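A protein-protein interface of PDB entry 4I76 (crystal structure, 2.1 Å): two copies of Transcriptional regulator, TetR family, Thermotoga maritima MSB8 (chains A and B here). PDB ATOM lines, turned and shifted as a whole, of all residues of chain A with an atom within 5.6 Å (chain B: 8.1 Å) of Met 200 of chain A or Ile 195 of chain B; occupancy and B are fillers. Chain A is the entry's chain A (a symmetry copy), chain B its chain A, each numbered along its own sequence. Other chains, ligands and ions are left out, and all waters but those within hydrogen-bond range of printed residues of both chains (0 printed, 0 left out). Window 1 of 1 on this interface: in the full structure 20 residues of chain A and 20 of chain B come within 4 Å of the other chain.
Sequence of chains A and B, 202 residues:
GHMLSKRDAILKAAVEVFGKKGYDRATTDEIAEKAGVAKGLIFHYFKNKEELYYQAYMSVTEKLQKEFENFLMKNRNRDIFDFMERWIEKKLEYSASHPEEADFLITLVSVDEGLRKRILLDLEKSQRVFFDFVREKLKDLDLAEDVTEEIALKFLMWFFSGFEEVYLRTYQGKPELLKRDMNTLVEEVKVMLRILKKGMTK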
ATOM      1  N   PHE A  81     -14.596 -15.760 -11.047  1.00  0.00           N
ATOM      2  CA  PHE A  81     -14.467 -16.684  -9.936  1.00  0.00           C
ATOM      3  C   PHE A  81     -15.167 -16.182  -8.694  1.00  0.00           C
ATOM      4  O   PHE A  81     -15.870 -16.972  -8.024  1.00  0.00           O
ATOM      5  CB  PHE A  81     -13.014 -16.963  -9.655  1.00  0.00           C
ATOM      6  CG  PHE A  81     -12.307 -17.469 -10.865  1.00  0.00           C
ATOM      7  CD1 PHE A  81     -12.434 -18.792 -11.254  1.00  0.00           C
ATOM      8  CD2 PHE A  81     -11.510 -16.610 -11.602  1.00  0.00           C
ATOM      9  CE1 PHE A  81     -11.791 -19.237 -12.409  1.00  0.00           C
ATOM     10  CE2 PHE A  81     -10.869 -17.045 -12.756  1.00  0.00           C
ATOM     11  CZ  PHE A  81     -11.033 -18.352 -13.170  1.00  0.00           C
ATOM     12  N   LEU A 138     -14.561 -14.866 -19.260  1.00  0.00           N
ATOM     13  CA  LEU A 138     -13.318 -15.583 -19.497  1.00  0.00           C
ATOM     14  C   LEU A 138     -12.395 -14.847 -20.442  1.00  0.00           C
ATOM     15  O   LEU A 138     -11.192 -14.844 -20.240  1.00  0.00           O
ATOM     16  CB  LEU A 138     -13.598 -17.020 -19.964  1.00  0.00           C
ATOM     17  CG  LEU A 138     -14.069 -17.983 -18.858  1.00  0.00           C
ATOM     18  CD1 LEU A 138     -14.406 -19.369 -19.423  1.00  0.00           C
ATOM     19  CD2 LEU A 138     -12.987 -18.114 -17.839  1.00  0.00           C
ATOM     20  N   ASP A 142      -6.399 -13.108 -18.544  1.00  0.00           N
ATOM     21  CA  ASP A 142      -5.212 -13.667 -19.158  1.00  0.00           C
ATOM     22  C   ASP A 142      -5.129 -15.134 -18.650  1.00  0.00           C
ATOM     23  O   ASP A 142      -4.798 -15.392 -17.488  1.00  0.00           O
ATOM     24  CB  ASP A 142      -3.959 -12.817 -18.837  1.00  0.00           C
ATOM     25  CG  ASP A 142      -3.872 -11.501 -19.692  1.00  0.00           C
ATOM     26  OD1 ASP A 142      -4.688 -11.328 -20.626  1.00  0.00           O
ATOM     27  OD2 ASP A 142      -2.987 -10.643 -19.445  1.00  0.00           O
ATOM     28  N   LEU A 143      -5.456 -16.074 -19.516  1.00  0.00           N
ATOM     29  CA  LEU A 143      -5.492 -17.498 -19.168  1.00  0.00           C
ATOM     30  C   LEU A 143      -4.099 -18.092 -19.110  1.00  0.00           C
ATOM     31  O   LEU A 143      -3.213 -17.658 -19.816  1.00  0.00           O
ATOM     32  CB  LEU A 143      -6.342 -18.304 -20.153  1.00  0.00           C
ATOM     33  CG  LEU A 143      -7.828 -17.966 -20.001  1.00  0.00           C
ATOM     34  CD1 LEU A 143      -8.633 -18.711 -21.041  1.00  0.00           C
ATOM     35  CD2 LEU A 143      -8.367 -18.288 -18.620  1.00  0.00           C
ATOM     36  N   ALA A 144      -3.919 -19.084 -18.245  1.00  0.00           N
ATOM     37  CA  ALA A 144      -2.635 -19.703 -18.072  1.00  0.00           C
ATOM     38  C   ALA A 144      -2.284 -20.510 -19.312  1.00  0.00           C
ATOM     39  O   ALA A 144      -3.118 -20.786 -20.127  1.00  0.00           O
ATOM     40  CB  ALA A 144      -2.668 -20.609 -16.857  1.00  0.00           C
ATOM     41  N   VAL A 147      -4.429 -23.405 -20.981  1.00  0.00           N
ATOM     42  CA  VAL A 147      -5.783 -23.323 -20.546  1.00  0.00           C
ATOM     43  C   VAL A 147      -6.511 -22.543 -21.658  1.00  0.00           C
ATOM     44  O   VAL A 147      -6.431 -21.328 -21.752  1.00  0.00           O
ATOM     45  CB  VAL A 147      -5.883 -22.613 -19.181  1.00  0.00           C
ATOM     46  CG1 VAL A 147      -7.350 -22.472 -18.780  1.00  0.00           C
ATOM     47  CG2 VAL A 147      -5.026 -23.386 -18.150  1.00  0.00           C
ATOM     48  N   ILE A 151     -11.716 -25.184 -22.493  1.00  0.00           N
ATOM     49  CA  ILE A 151     -11.460 -26.015 -21.287  1.00  0.00           C
ATOM     50  C   ILE A 151     -11.882 -25.239 -19.997  1.00  0.00           C
ATOM     51  O   ILE A 151     -12.492 -25.762 -19.131  1.00  0.00           O
ATOM     52  CB  ILE A 151      -9.998 -26.382 -21.207  1.00  0.00           C
ATOM     53  CG1 ILE A 151      -9.647 -27.396 -22.369  1.00  0.00           C
ATOM     54  CG2 ILE A 151      -9.724 -27.077 -19.917  1.00  0.00           C
ATOM     55  CD1 ILE A 151      -8.172 -27.673 -22.540  1.00  0.00           C
ATOM     56  N   ALA A 152     -11.479 -24.018 -19.886  1.00  0.00           N
ATOM     57  CA  ALA A 152     -11.857 -23.182 -18.712  1.00  0.00           C
ATOM     58  C   ALA A 152     -13.339 -23.188 -18.514  1.00  0.00           C
ATOM     59  O   ALA A 152     -13.820 -23.442 -17.443  1.00  0.00           O
ATOM     60  CB  ALA A 152     -11.333 -21.758 -18.930  1.00  0.00           C
ATOM     61  N   PHE A 155     -14.812 -26.814 -17.565  1.00  0.00           N
ATOM     62  CA  PHE A 155     -14.452 -27.157 -16.198  1.00  0.00           C
ATOM     63  C   PHE A 155     -15.295 -26.314 -15.218  1.00  0.00           C
ATOM     64  O   PHE A 155     -15.832 -26.851 -14.286  1.00  0.00           O
ATOM     65  CB  PHE A 155     -12.964 -26.883 -16.017  1.00  0.00           C
ATOM     66  CG  PHE A 155     -12.279 -27.633 -14.905  1.00  0.00           C
ATOM     67  CD1 PHE A 155     -12.945 -28.459 -14.036  1.00  0.00           C
ATOM     68  CD2 PHE A 155     -10.920 -27.399 -14.691  1.00  0.00           C
ATOM     69  CE1 PHE A 155     -12.233 -29.116 -13.028  1.00  0.00           C
ATOM     70  CE2 PHE A 155     -10.221 -28.035 -13.662  1.00  0.00           C
ATOM     71  CZ  PHE A 155     -10.861 -28.938 -12.879  1.00  0.00           C
ATOM     72  N   LEU A 156     -15.417 -25.011 -15.457  1.00  0.00           N
ATOM     73  CA  LEU A 156     -16.189 -24.162 -14.574  1.00  0.00           C
ATOM     74  C   LEU A 156     -17.660 -24.528 -14.561  1.00  0.00           C
ATOM     75  O   LEU A 156     -18.305 -24.464 -13.495  1.00  0.00           O
ATOM     76  CB  LEU A 156     -16.001 -22.684 -14.945  1.00  0.00           C
ATOM     77  CG  LEU A 156     -14.698 -21.987 -14.577  1.00  0.00           C
ATOM     78  CD1 LEU A 156     -14.749 -20.522 -15.058  1.00  0.00           C
ATOM     79  CD2 LEU A 156     -14.470 -22.100 -13.062  1.00  0.00           C
ATOM     80  N   ILE A 195      -8.778 -22.126  -5.996  1.00  0.00           N
ATOM     81  CA  ILE A 195      -7.872 -23.179  -6.606  1.00  0.00           C
ATOM     82  C   ILE A 195      -7.973 -23.024  -8.137  1.00  0.00           C
ATOM     83  O   ILE A 195      -6.987 -22.876  -8.820  1.00  0.00           O
ATOM     84  CB  ILE A 195      -8.264 -24.592  -6.147  1.00  0.00           C
ATOM     85  CG1 ILE A 195      -7.805 -24.849  -4.705  1.00  0.00           C
ATOM     86  CG2 ILE A 195      -7.597 -25.674  -7.019  1.00  0.00           C
ATOM     87  CD1 ILE A 195      -8.514 -25.998  -4.004  1.00  0.00           C
ATOM     88  N   LEU A 196      -9.207 -22.927  -8.628  1.00  0.00           N
ATOM     89  CA  LEU A 196      -9.461 -22.845 -10.075  1.00  0.00           C
ATOM     90  C   LEU A 196      -8.973 -21.543 -10.677  1.00  0.00           C
ATOM     91  O   LEU A 196      -8.328 -21.549 -11.733  1.00  0.00           O
ATOM     92  CB  LEU A 196     -10.943 -23.031 -10.364  1.00  0.00           C
ATOM     93  CG  LEU A 196     -11.431 -24.487 -10.169  1.00  0.00           C
ATOM     94  CD1 LEU A 196     -12.929 -24.495 -10.322  1.00  0.00           C
ATOM     95  CD2 LEU A 196     -10.825 -25.500 -11.140  1.00  0.00           C
ATOM     96  N   LYS A 197      -9.202 -20.441  -9.981  1.00  0.00           N
ATOM     97  CA  LYS A 197      -8.620 -19.205 -10.417  1.00  0.00           C
ATOM     98  C   LYS A 197      -7.055 -19.201 -10.571  1.00  0.00           C
ATOM     99  O   LYS A 197      -6.486 -18.711 -11.595  1.00  0.00           O
ATOM    100  CB  LYS A 197      -9.005 -18.093  -9.462  1.00  0.00           C
ATOM    101  CG  LYS A 197      -8.366 -16.763  -9.834  1.00  0.00           C
ATOM    102  CD  LYS A 197      -8.921 -15.592  -8.963  1.00  0.00           C
ATOM    103  CE  LYS A 197      -8.091 -14.338  -9.227  1.00  0.00           C
ATOM    104  NZ  LYS A 197      -8.508 -13.269  -8.288  1.00  0.00           N
ATOM    105  N   LYS A 198      -6.389 -19.629  -9.506  1.00  0.00           N
ATOM    106  CA  LYS A 198      -4.947 -19.710  -9.513  1.00  0.00           C
ATOM    107  C   LYS A 198      -4.435 -20.658 -10.628  1.00  0.00           C
ATOM    108  O   LYS A 198      -3.418 -20.391 -11.210  1.00  0.00           O
ATOM    109  CB  LYS A 198      -4.436 -20.150  -8.125  1.00  0.00           C
ATOM    110  CG  LYS A 198      -2.961 -20.477  -8.063  1.00  0.00           C
ATOM    111  CD  LYS A 198      -2.352 -20.131  -6.702  1.00  0.00           C
ATOM    112  CE  LYS A 198      -1.362 -21.199  -6.216  1.00  0.00           C
ATOM    113  NZ  LYS A 198      -0.730 -20.902  -4.879  1.00  0.00           N
ATOM    114  N   GLY A 199      -5.139 -21.749 -10.884  1.00  0.00           N
ATOM    115  CA  GLY A 199      -4.686 -22.731 -11.855  1.00  0.00           C
ATOM    116  C   GLY A 199      -4.987 -22.353 -13.304  1.00  0.00           C
ATOM    117  O   GLY A 199      -4.264 -22.736 -14.188  1.00  0.00           O
ATOM    118  N   MET A 200      -6.050 -21.582 -13.511  1.00  0.00           N
ATOM    119  CA  MET A 200      -6.532 -21.244 -14.822  1.00  0.00           C
ATOM    120  C   MET A 200      -5.929 -19.995 -15.357  1.00  0.00           C
ATOM    121  O   MET A 200      -5.831 -19.819 -16.574  1.00  0.00           O
ATOM    122  CB  MET A 200      -8.022 -20.964 -14.800  1.00  0.00           C
ATOM    123  CG  MET A 200      -8.743 -22.275 -14.654  1.00  0.00           C
ATOM    124  SD  MET A 200     -10.695 -21.977 -14.874  1.00  0.00           S
ATOM    125  CE  MET A 200     -11.319 -23.820 -14.632  1.00  0.00           C
ATOM    126  N   THR A 201      -5.493 -19.116 -14.484  1.00  0.00           N
ATOM    127  CA  THR A 201      -4.997 -17.820 -14.939  1.00  0.00           C
ATOM    128  C   THR A 201      -3.495 -17.711 -14.836  1.00  0.00           C
ATOM    129  O   THR A 201      -2.845 -18.409 -14.091  1.00  0.00           O
ATOM    130  CB  THR A 201      -5.650 -16.628 -14.171  1.00  0.00           C
ATOM    131  OG1 THR A 201      -5.251 -16.667 -12.810  1.00  0.00           O
ATOM    132  CG2 THR A 201      -7.145 -16.678 -14.287  1.00  0.00           C
ATOM    133  N   LYS A 202      -2.944 -16.761 -15.577  1.00  0.00           N
ATOM    134  CA  LYS A 202      -1.514 -16.571 -15.632  1.00  0.00           C
ATOM    135  C   LYS A 202      -1.077 -15.891 -14.342  1.00  0.00           C
ATOM    136  O   LYS A 202      -1.818 -15.076 -13.789  1.00  0.00           O
ATOM    137  CB  LYS A 202      -1.231 -15.733 -16.878  1.00  0.00           C
ATOM    138  CG  LYS A 202       0.150 -15.846 -17.423  1.00  0.00           C
ATOM    139  CD  LYS A 202       0.215 -15.347 -18.848  1.00  0.00           C
ATOM    140  CE  LYS A 202       0.288 -16.535 -19.793  1.00  0.00           C
ATOM    141  NZ  LYS A 202       0.796 -16.136 -21.134  1.00  0.00           N
ATOM    142  OXT LYS A 202      -0.017 -16.162 -13.752  1.00  0.00           O
ATOM    143  N   PHE B  81      -1.226 -35.816  -9.096  1.00  0.00           N
ATOM    144  CA  PHE B  81      -1.900 -35.262 -10.254  1.00  0.00           C
ATOM    145  C   PHE B  81      -1.547 -35.998 -11.525  1.00  0.00           C
ATOM    146  O   PHE B  81      -2.455 -36.295 -12.334  1.00  0.00           O
ATOM    147  CB  PHE B  81      -1.591 -33.792 -10.382  1.00  0.00           C
ATOM    148  CG  PHE B  81      -1.940 -33.046  -9.142  1.00  0.00           C
ATOM    149  CD1 PHE B  81      -3.254 -32.694  -8.877  1.00  0.00           C
ATOM    150  CD2 PHE B  81      -0.942 -32.692  -8.250  1.00  0.00           C
ATOM    151  CE1 PHE B  81      -3.564 -32.025  -7.694  1.00  0.00           C
ATOM    152  CE2 PHE B  81      -1.244 -32.029  -7.068  1.00  0.00           C
ATOM    153  CZ  PHE B  81      -2.559 -31.721  -6.780  1.00  0.00           C
ATOM    154  N   PHE B 155     -12.271 -32.365  -3.548  1.00  0.00           N
ATOM    155  CA  PHE B 155     -12.295 -31.796  -4.885  1.00  0.00           C
ATOM    156  C   PHE B 155     -11.712 -32.813  -5.888  1.00  0.00           C
ATOM    157  O   PHE B 155     -12.295 -33.032  -6.916  1.00  0.00           O
ATOM    158  CB  PHE B 155     -11.475 -30.511  -4.867  1.00  0.00           C
ATOM    159  CG  PHE B 155     -11.785 -29.508  -5.947  1.00  0.00           C
ATOM    160  CD1 PHE B 155     -12.690 -29.742  -6.952  1.00  0.00           C
ATOM    161  CD2 PHE B 155     -11.045 -28.325  -5.981  1.00  0.00           C
ATOM    162  CE1 PHE B 155     -12.915 -28.757  -7.917  1.00  0.00           C
ATOM    163  CE2 PHE B 155     -11.254 -27.358  -6.967  1.00  0.00           C
ATOM    164  CZ  PHE B 155     -12.230 -27.546  -7.890  1.00  0.00           C
ATOM    165  N   PHE B 159     -13.730 -34.660  -8.902  1.00  0.00           N
ATOM    166  CA  PHE B 159     -13.210 -34.607 -10.260  1.00  0.00           C
ATOM    167  C   PHE B 159     -13.158 -36.026 -10.813  1.00  0.00           C
ATOM    168  O   PHE B 159     -13.715 -36.293 -11.876  1.00  0.00           O
ATOM    169  CB  PHE B 159     -11.826 -33.924 -10.330  1.00  0.00           C
ATOM    170  CG  PHE B 159     -11.191 -33.922 -11.725  1.00  0.00           C
ATOM    171  CD1 PHE B 159     -10.255 -34.882 -12.080  1.00  0.00           C
ATOM    172  CD2 PHE B 159     -11.486 -32.924 -12.660  1.00  0.00           C
ATOM    173  CE1 PHE B 159      -9.672 -34.897 -13.348  1.00  0.00           C
ATOM    174  CE2 PHE B 159     -10.903 -32.932 -13.929  1.00  0.00           C
ATOM    175  CZ  PHE B 159     -10.000 -33.922 -14.271  1.00  0.00           C
ATOM    176  N   GLU B 188      -7.537 -32.784 -22.599  1.00  0.00           N
ATOM    177  CA  GLU B 188      -8.298 -31.916 -21.665  1.00  0.00           C
ATOM    178  C   GLU B 188      -8.141 -32.334 -20.207  1.00  0.00           C
ATOM    179  O   GLU B 188      -8.007 -31.515 -19.338  1.00  0.00           O
ATOM    180  CB  GLU B 188      -9.785 -31.963 -22.011  1.00  0.00           C
ATOM    181  CG  GLU B 188     -10.070 -31.293 -23.343  1.00  0.00           C
ATOM    182  CD  GLU B 188     -11.536 -31.269 -23.674  1.00  0.00           C
ATOM    183  OE1 GLU B 188     -12.241 -32.191 -23.239  1.00  0.00           O
ATOM    184  OE2 GLU B 188     -11.957 -30.342 -24.397  1.00  0.00           O
ATOM    185  N   VAL B 189      -8.111 -33.628 -19.955  1.00  0.00           N
ATOM    186  CA  VAL B 189      -7.853 -34.117 -18.595  1.00  0.00           C
ATOM    187  C   VAL B 189      -6.507 -33.691 -18.082  1.00  0.00           C
ATOM    188  O   VAL B 189      -6.340 -33.239 -16.925  1.00  0.00           O
ATOM    189  CB  VAL B 189      -8.055 -35.639 -18.478  1.00  0.00           C
ATOM    190  CG1 VAL B 189      -7.664 -36.143 -17.080  1.00  0.00           C
ATOM    191  CG2 VAL B 189      -9.478 -35.989 -18.778  1.00  0.00           C
ATOM    192  N   LYS B 190      -5.515 -33.774 -18.942  1.00  0.00           N
ATOM    193  CA  LYS B 190      -4.198 -33.292 -18.517  1.00  0.00           C
ATOM    194  C   LYS B 190      -4.247 -31.811 -18.098  1.00  0.00           C
ATOM    195  O   LYS B 190      -3.587 -31.396 -17.148  1.00  0.00           O
ATOM    196  CB  LYS B 190      -3.197 -33.428 -19.636  1.00  0.00           C
ATOM    197  CG  LYS B 190      -2.780 -34.894 -19.924  1.00  0.00           C
ATOM    198  CD  LYS B 190      -1.877 -34.945 -21.149  1.00  0.00           C
ATOM    199  CE  LYS B 190      -1.368 -36.367 -21.429  1.00  0.00           C
ATOM    200  NZ  LYS B 190      -0.766 -36.440 -22.777  1.00  0.00           N
ATOM    201  N   VAL B 191      -4.897 -30.990 -18.899  1.00  0.00           N
ATOM    202  CA  VAL B 191      -4.893 -29.524 -18.576  1.00  0.00           C
ATOM    203  C   VAL B 191      -5.667 -29.273 -17.271  1.00  0.00           C
ATOM    204  O   VAL B 191      -5.295 -28.441 -16.467  1.00  0.00           O
ATOM    205  CB  VAL B 191      -5.508 -28.733 -19.725  1.00  0.00           C
ATOM    206  CG1 VAL B 191      -5.771 -27.286 -19.276  1.00  0.00           C
ATOM    207  CG2 VAL B 191      -4.573 -28.800 -20.937  1.00  0.00           C
ATOM    208  N   MET B 192      -6.764 -29.987 -17.095  1.00  0.00           N
ATOM    209  CA  MET B 192      -7.590 -29.804 -15.917  1.00  0.00           C
ATOM    210  C   MET B 192      -6.870 -30.207 -14.667  1.00  0.00           C
ATOM    211  O   MET B 192      -7.036 -29.569 -13.607  1.00  0.00           O
ATOM    212  CB  MET B 192      -8.883 -30.593 -16.094  1.00  0.00           C
ATOM    213  CG  MET B 192      -9.827 -29.903 -17.068  1.00  0.00           C
ATOM    214  SD  MET B 192     -11.411 -31.046 -17.379  1.00  0.00           S
ATOM    215  CE  MET B 192     -12.264 -30.075 -18.903  1.00  0.00           C
ATOM    216  N   LEU B 193      -6.104 -31.293 -14.759  1.00  0.00           N
ATOM    217  CA  LEU B 193      -5.269 -31.720 -13.628  1.00  0.00           C
ATOM    218  C   LEU B 193      -4.090 -30.815 -13.409  1.00  0.00           C
ATOM    219  O   LEU B 193      -3.685 -30.596 -12.273  1.00  0.00           O
ATOM    220  CB  LEU B 193      -4.778 -33.159 -13.755  1.00  0.00           C
ATOM    221  CG  LEU B 193      -5.423 -34.301 -12.948  1.00  0.00           C
ATOM    222  CD1 LEU B 193      -6.240 -34.002 -11.674  1.00  0.00           C
ATOM    223  CD2 LEU B 193      -6.115 -35.307 -13.824  1.00  0.00           C
ATOM    224  N   ARG B 194      -3.504 -30.292 -14.463  1.00  0.00           N
ATOM    225  CA  ARG B 194      -2.497 -29.263 -14.258  1.00  0.00           C
ATOM    226  C   ARG B 194      -3.147 -28.004 -13.563  1.00  0.00           C
ATOM    227  O   ARG B 194      -2.484 -27.334 -12.819  1.00  0.00           O
ATOM    228  CB  ARG B 194      -1.835 -28.851 -15.571  1.00  0.00           C
ATOM    229  CG  ARG B 194      -0.813 -29.894 -16.066  1.00  0.00           C
ATOM    230  CD  ARG B 194      -0.427 -29.683 -17.504  1.00  0.00           C
ATOM    231  NE  ARG B 194       0.057 -28.320 -17.724  1.00  0.00           N
ATOM    232  CZ  ARG B 194       0.119 -27.715 -18.911  1.00  0.00           C
ATOM    233  NH1 ARG B 194      -0.285 -28.341 -20.042  1.00  0.00           N
ATOM    234  NH2 ARG B 194       0.574 -26.463 -18.970  1.00  0.00           N
ATOM    235  N   ILE B 195      -4.370 -27.646 -13.917  1.00  0.00           N
ATOM    236  CA  ILE B 195      -5.081 -26.461 -13.289  1.00  0.00           C
ATOM    237  C   ILE B 195      -5.155 -26.735 -11.773  1.00  0.00           C
ATOM    238  O   ILE B 195      -4.737 -25.935 -10.970  1.00  0.00           O
ATOM    239  CB  ILE B 195      -6.475 -26.253 -13.902  1.00  0.00           C
ATOM    240  CG1 ILE B 195      -6.373 -25.619 -15.296  1.00  0.00           C
ATOM    241  CG2 ILE B 195      -7.330 -25.299 -13.046  1.00  0.00           C
ATOM    242  CD1 ILE B 195      -7.611 -25.784 -16.164  1.00  0.00           C
ATOM    243  N   LEU B 196      -5.576 -27.949 -11.425  1.00  0.00           N
ATOM    244  CA  LEU B 196      -5.764 -28.329 -10.016  1.00  0.00           C
ATOM    245  C   LEU B 196      -4.454 -28.418  -9.259  1.00  0.00           C
ATOM    246  O   LEU B 196      -4.347 -27.904  -8.138  1.00  0.00           O
ATOM    247  CB  LEU B 196      -6.514 -29.650  -9.920  1.00  0.00           C
ATOM    248  CG  LEU B 196      -8.013 -29.535 -10.285  1.00  0.00           C
ATOM    249  CD1 LEU B 196      -8.588 -30.927 -10.311  1.00  0.00           C
ATOM    250  CD2 LEU B 196      -8.840 -28.671  -9.333  1.00  0.00           C
ATOM    251  N   LYS B 197      -3.439 -28.990  -9.888  1.00  0.00           N
ATOM    252  CA  LYS B 197      -2.136 -28.954  -9.289  1.00  0.00           C
ATOM    253  C   LYS B 197      -1.577 -27.523  -8.953  1.00  0.00           C
ATOM    254  O   LYS B 197      -1.036 -27.264  -7.833  1.00  0.00           O
ATOM    255  CB  LYS B 197      -1.140 -29.652 -10.192  1.00  0.00           C
ATOM    256  CG  LYS B 197       0.278 -29.594  -9.643  1.00  0.00           C
ATOM    257  CD  LYS B 197       1.258 -30.478 -10.477  1.00  0.00           C
ATOM    258  CE  LYS B 197       2.688 -30.206 -10.018  1.00  0.00           C
ATOM    259  NZ  LYS B 197       3.633 -30.919 -10.912  1.00  0.00           N
ATOM    260  N   LYS B 198      -1.602 -26.662  -9.962  1.00  0.00           N
ATOM    261  CA  LYS B 198      -1.149 -25.301  -9.792  1.00  0.00           C
ATOM    262  C   LYS B 198      -1.966 -24.560  -8.704  1.00  0.00           C
ATOM    263  O   LYS B 198      -1.416 -23.769  -7.986  1.00  0.00           O
ATOM    264  CB  LYS B 198      -1.203 -24.554 -11.141  1.00  0.00           C
ATOM    265  CG  LYS B 198      -0.957 -23.065 -11.055  1.00  0.00           C
ATOM    266  CD  LYS B 198      -0.253 -22.525 -12.303  1.00  0.00           C
ATOM    267  CE  LYS B 198      -0.819 -21.170 -12.752  1.00  0.00           C
ATOM    268  NZ  LYS B 198      -0.155 -20.593 -13.978  1.00  0.00           N
ATOM    269  N   GLY B 199      -3.261 -24.819  -8.619  1.00  0.00           N
ATOM    270  CA  GLY B 199      -4.116 -24.108  -7.683  1.00  0.00           C
ATOM    271  C   GLY B 199      -4.048 -24.643  -6.254  1.00  0.00           C
ATOM    272  O   GLY B 199      -4.241 -23.902  -5.325  1.00  0.00           O
ATOM    273  N   MET B 200      -3.751 -25.931  -6.113  1.00  0.00           N
ATOM    274  CA  MET B 200      -3.770 -26.607  -4.845  1.00  0.00           C
ATOM    275  C   MET B 200      -2.460 -26.565  -4.145  1.00  0.00           C
ATOM    276  O   MET B 200      -2.404 -26.637  -2.915  1.00  0.00           O
ATOM    277  CB  MET B 200      -4.057 -28.087  -5.020  1.00  0.00           C
ATOM    278  CG  MET B 200      -5.514 -28.246  -5.354  1.00  0.00           C
ATOM    279  SD  MET B 200      -5.981 -30.176  -5.342  1.00  0.00           S
ATOM    280  CE  MET B 200      -7.882 -30.038  -5.801  1.00  0.00           C
ATOM    281  N   THR B 201      -1.386 -26.425  -4.889  1.00  0.00           N
ATOM    282  CA  THR B 201      -0.062 -26.492  -4.276  1.00  0.00           C
ATOM    283  C   THR B 201       0.602 -25.139  -4.193  1.00  0.00           C
ATOM    284  O   THR B 201       0.285 -24.217  -4.909  1.00  0.00           O
ATOM    285  CB  THR B 201       0.889 -27.483  -5.019  1.00  0.00           C
ATOM    286  OG1 THR B 201       1.160 -26.992  -6.323  1.00  0.00           O
ATOM    287  CG2 THR B 201       0.281 -28.852  -5.084  1.00  0.00           C
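Of the printed residues of chain B, Val 147 of chain A touches Ile 195. Ala 152 of chain A touches none of the printed residues of chain B. Of the printed residues of chain B, Phe 155 of chain A touches Phe 159, Met 192, Ile 195 and Leu 196. Printed residues of chain B within 4 Å of Leu 196 of chain A: Phe 155 and Ile 195. Of the printed residues of chain B, Lys 198 of chain A touches Lys 198 (3.1 Å), Gly 199 (3.8 Å) and Thr 201 (3.5 Å). Gly 199 of chain A touches just these residues of chain B: Ile 195 (3.3 Å) and Lys 198 (3.8 Å). Met 200 of chain A touches just one residue of chain B: Ile 195. Glu 188 of chain B touches none of the printed residues of chain A. Printed residues of chain A within 4 Å of Met 192 of chain B: Phe 155. Of the printed residues of chain A, Ile 195 of chain B touches Val 147 (3.9 Å), Phe 155 (3.97 Å), Leu 196 (3.99 Å), Gly 199 (3.3 Å) and Met 200 (3.7 Å).
Among the printed residues, merely in contact across the chains: Lys 198 of chain A with Lys 198 of chain B (3.1 Å), Gly 199 of chain A with Ile 195 of chain B (3.3 Å), Ile 195 of chain A with Gly 199 of chain B (3.3 Å), Phe 155 of chain A with Met 192 of chain B (3.5 Å), Ile 195 of chain A with Met 200 of chain B (3.7 Å), Met 200 of chain A with Ile 195 of chain B (3.7 Å), Ala 144 of chain A with Lys 198 of chain B (3.8 Å), Gly 199 of chain A with Lys 198 of chain B (3.8 Å), Lys 198 of chain A with Gly 199 of chain B (3.8 Å), Val 147 of chain A with Ile 195 of chain B (3.9 Å), Leu 196 of chain A with Phe 155 of chain B (3.9 Å), Phe 155 of chain A with Phe 159 of chain B (3.9 Å), Phe 155 of chain A with Leu 196 of chain B (3.9 Å), Phe 155 of chain A with Ile 195 of chain B (3.97 Å), Ile 195 of chain A with Phe 155 of chain B (3.97 Å), Ile 195 of chain A with Leu 196 of chain B (3.99 Å) and Leu 196 of chain A with Ile 195 of chain B (3.99 Å).
The backbone carbonyl oxygen (O) of Thr 201 of chain A is in hydrogen-bond range of the side-chain amino group (NZ) of Lys 198 of chain B, 3.5 Å away. The backbone carbonyl oxygen of Thr 201 of chain B lies within hydrogen-bond range of the side-chain amino group of Lys 198 of chain A, 3.5 Å away.
Of the 18 printed residues of chain A, 9 touch a printed residue of chain B. Among the printed residues, 19 pairs touch across the chains.
OG1 of Thr 201 of chain B sits at hydrogen-bond distance from O of Lys 197 of chain B (2.7 Å). O of Met 200 of chain A lies within hydrogen-bond range of N of Ala 144 of chain A, at 2.6 Å. The backbone carbonyl oxygen of Lys 197 of chain A is in hydrogen-bond range of the side-chain hydroxyl of Thr 201 of chain A.
Phe 155 of chain A touches Ile 195 of chain B, and with the chains exchanged Ile 195 of chain A touches Phe 155 of chain B. Phe 155 of chain A touches Leu 196 of chain B, and with the chains exchanged Leu 196 of chain A touches Phe 155 of chain B. Ile 195 of chain A touches Leu 196 of chain B, and with the chains exchanged Leu 196 of chain A touches Ile 195 of chain B. Lys 198 of chain A touches Thr 201 of chain B, and with the chains exchanged Thr 201 of chain A touches Lys 198 of chain B.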
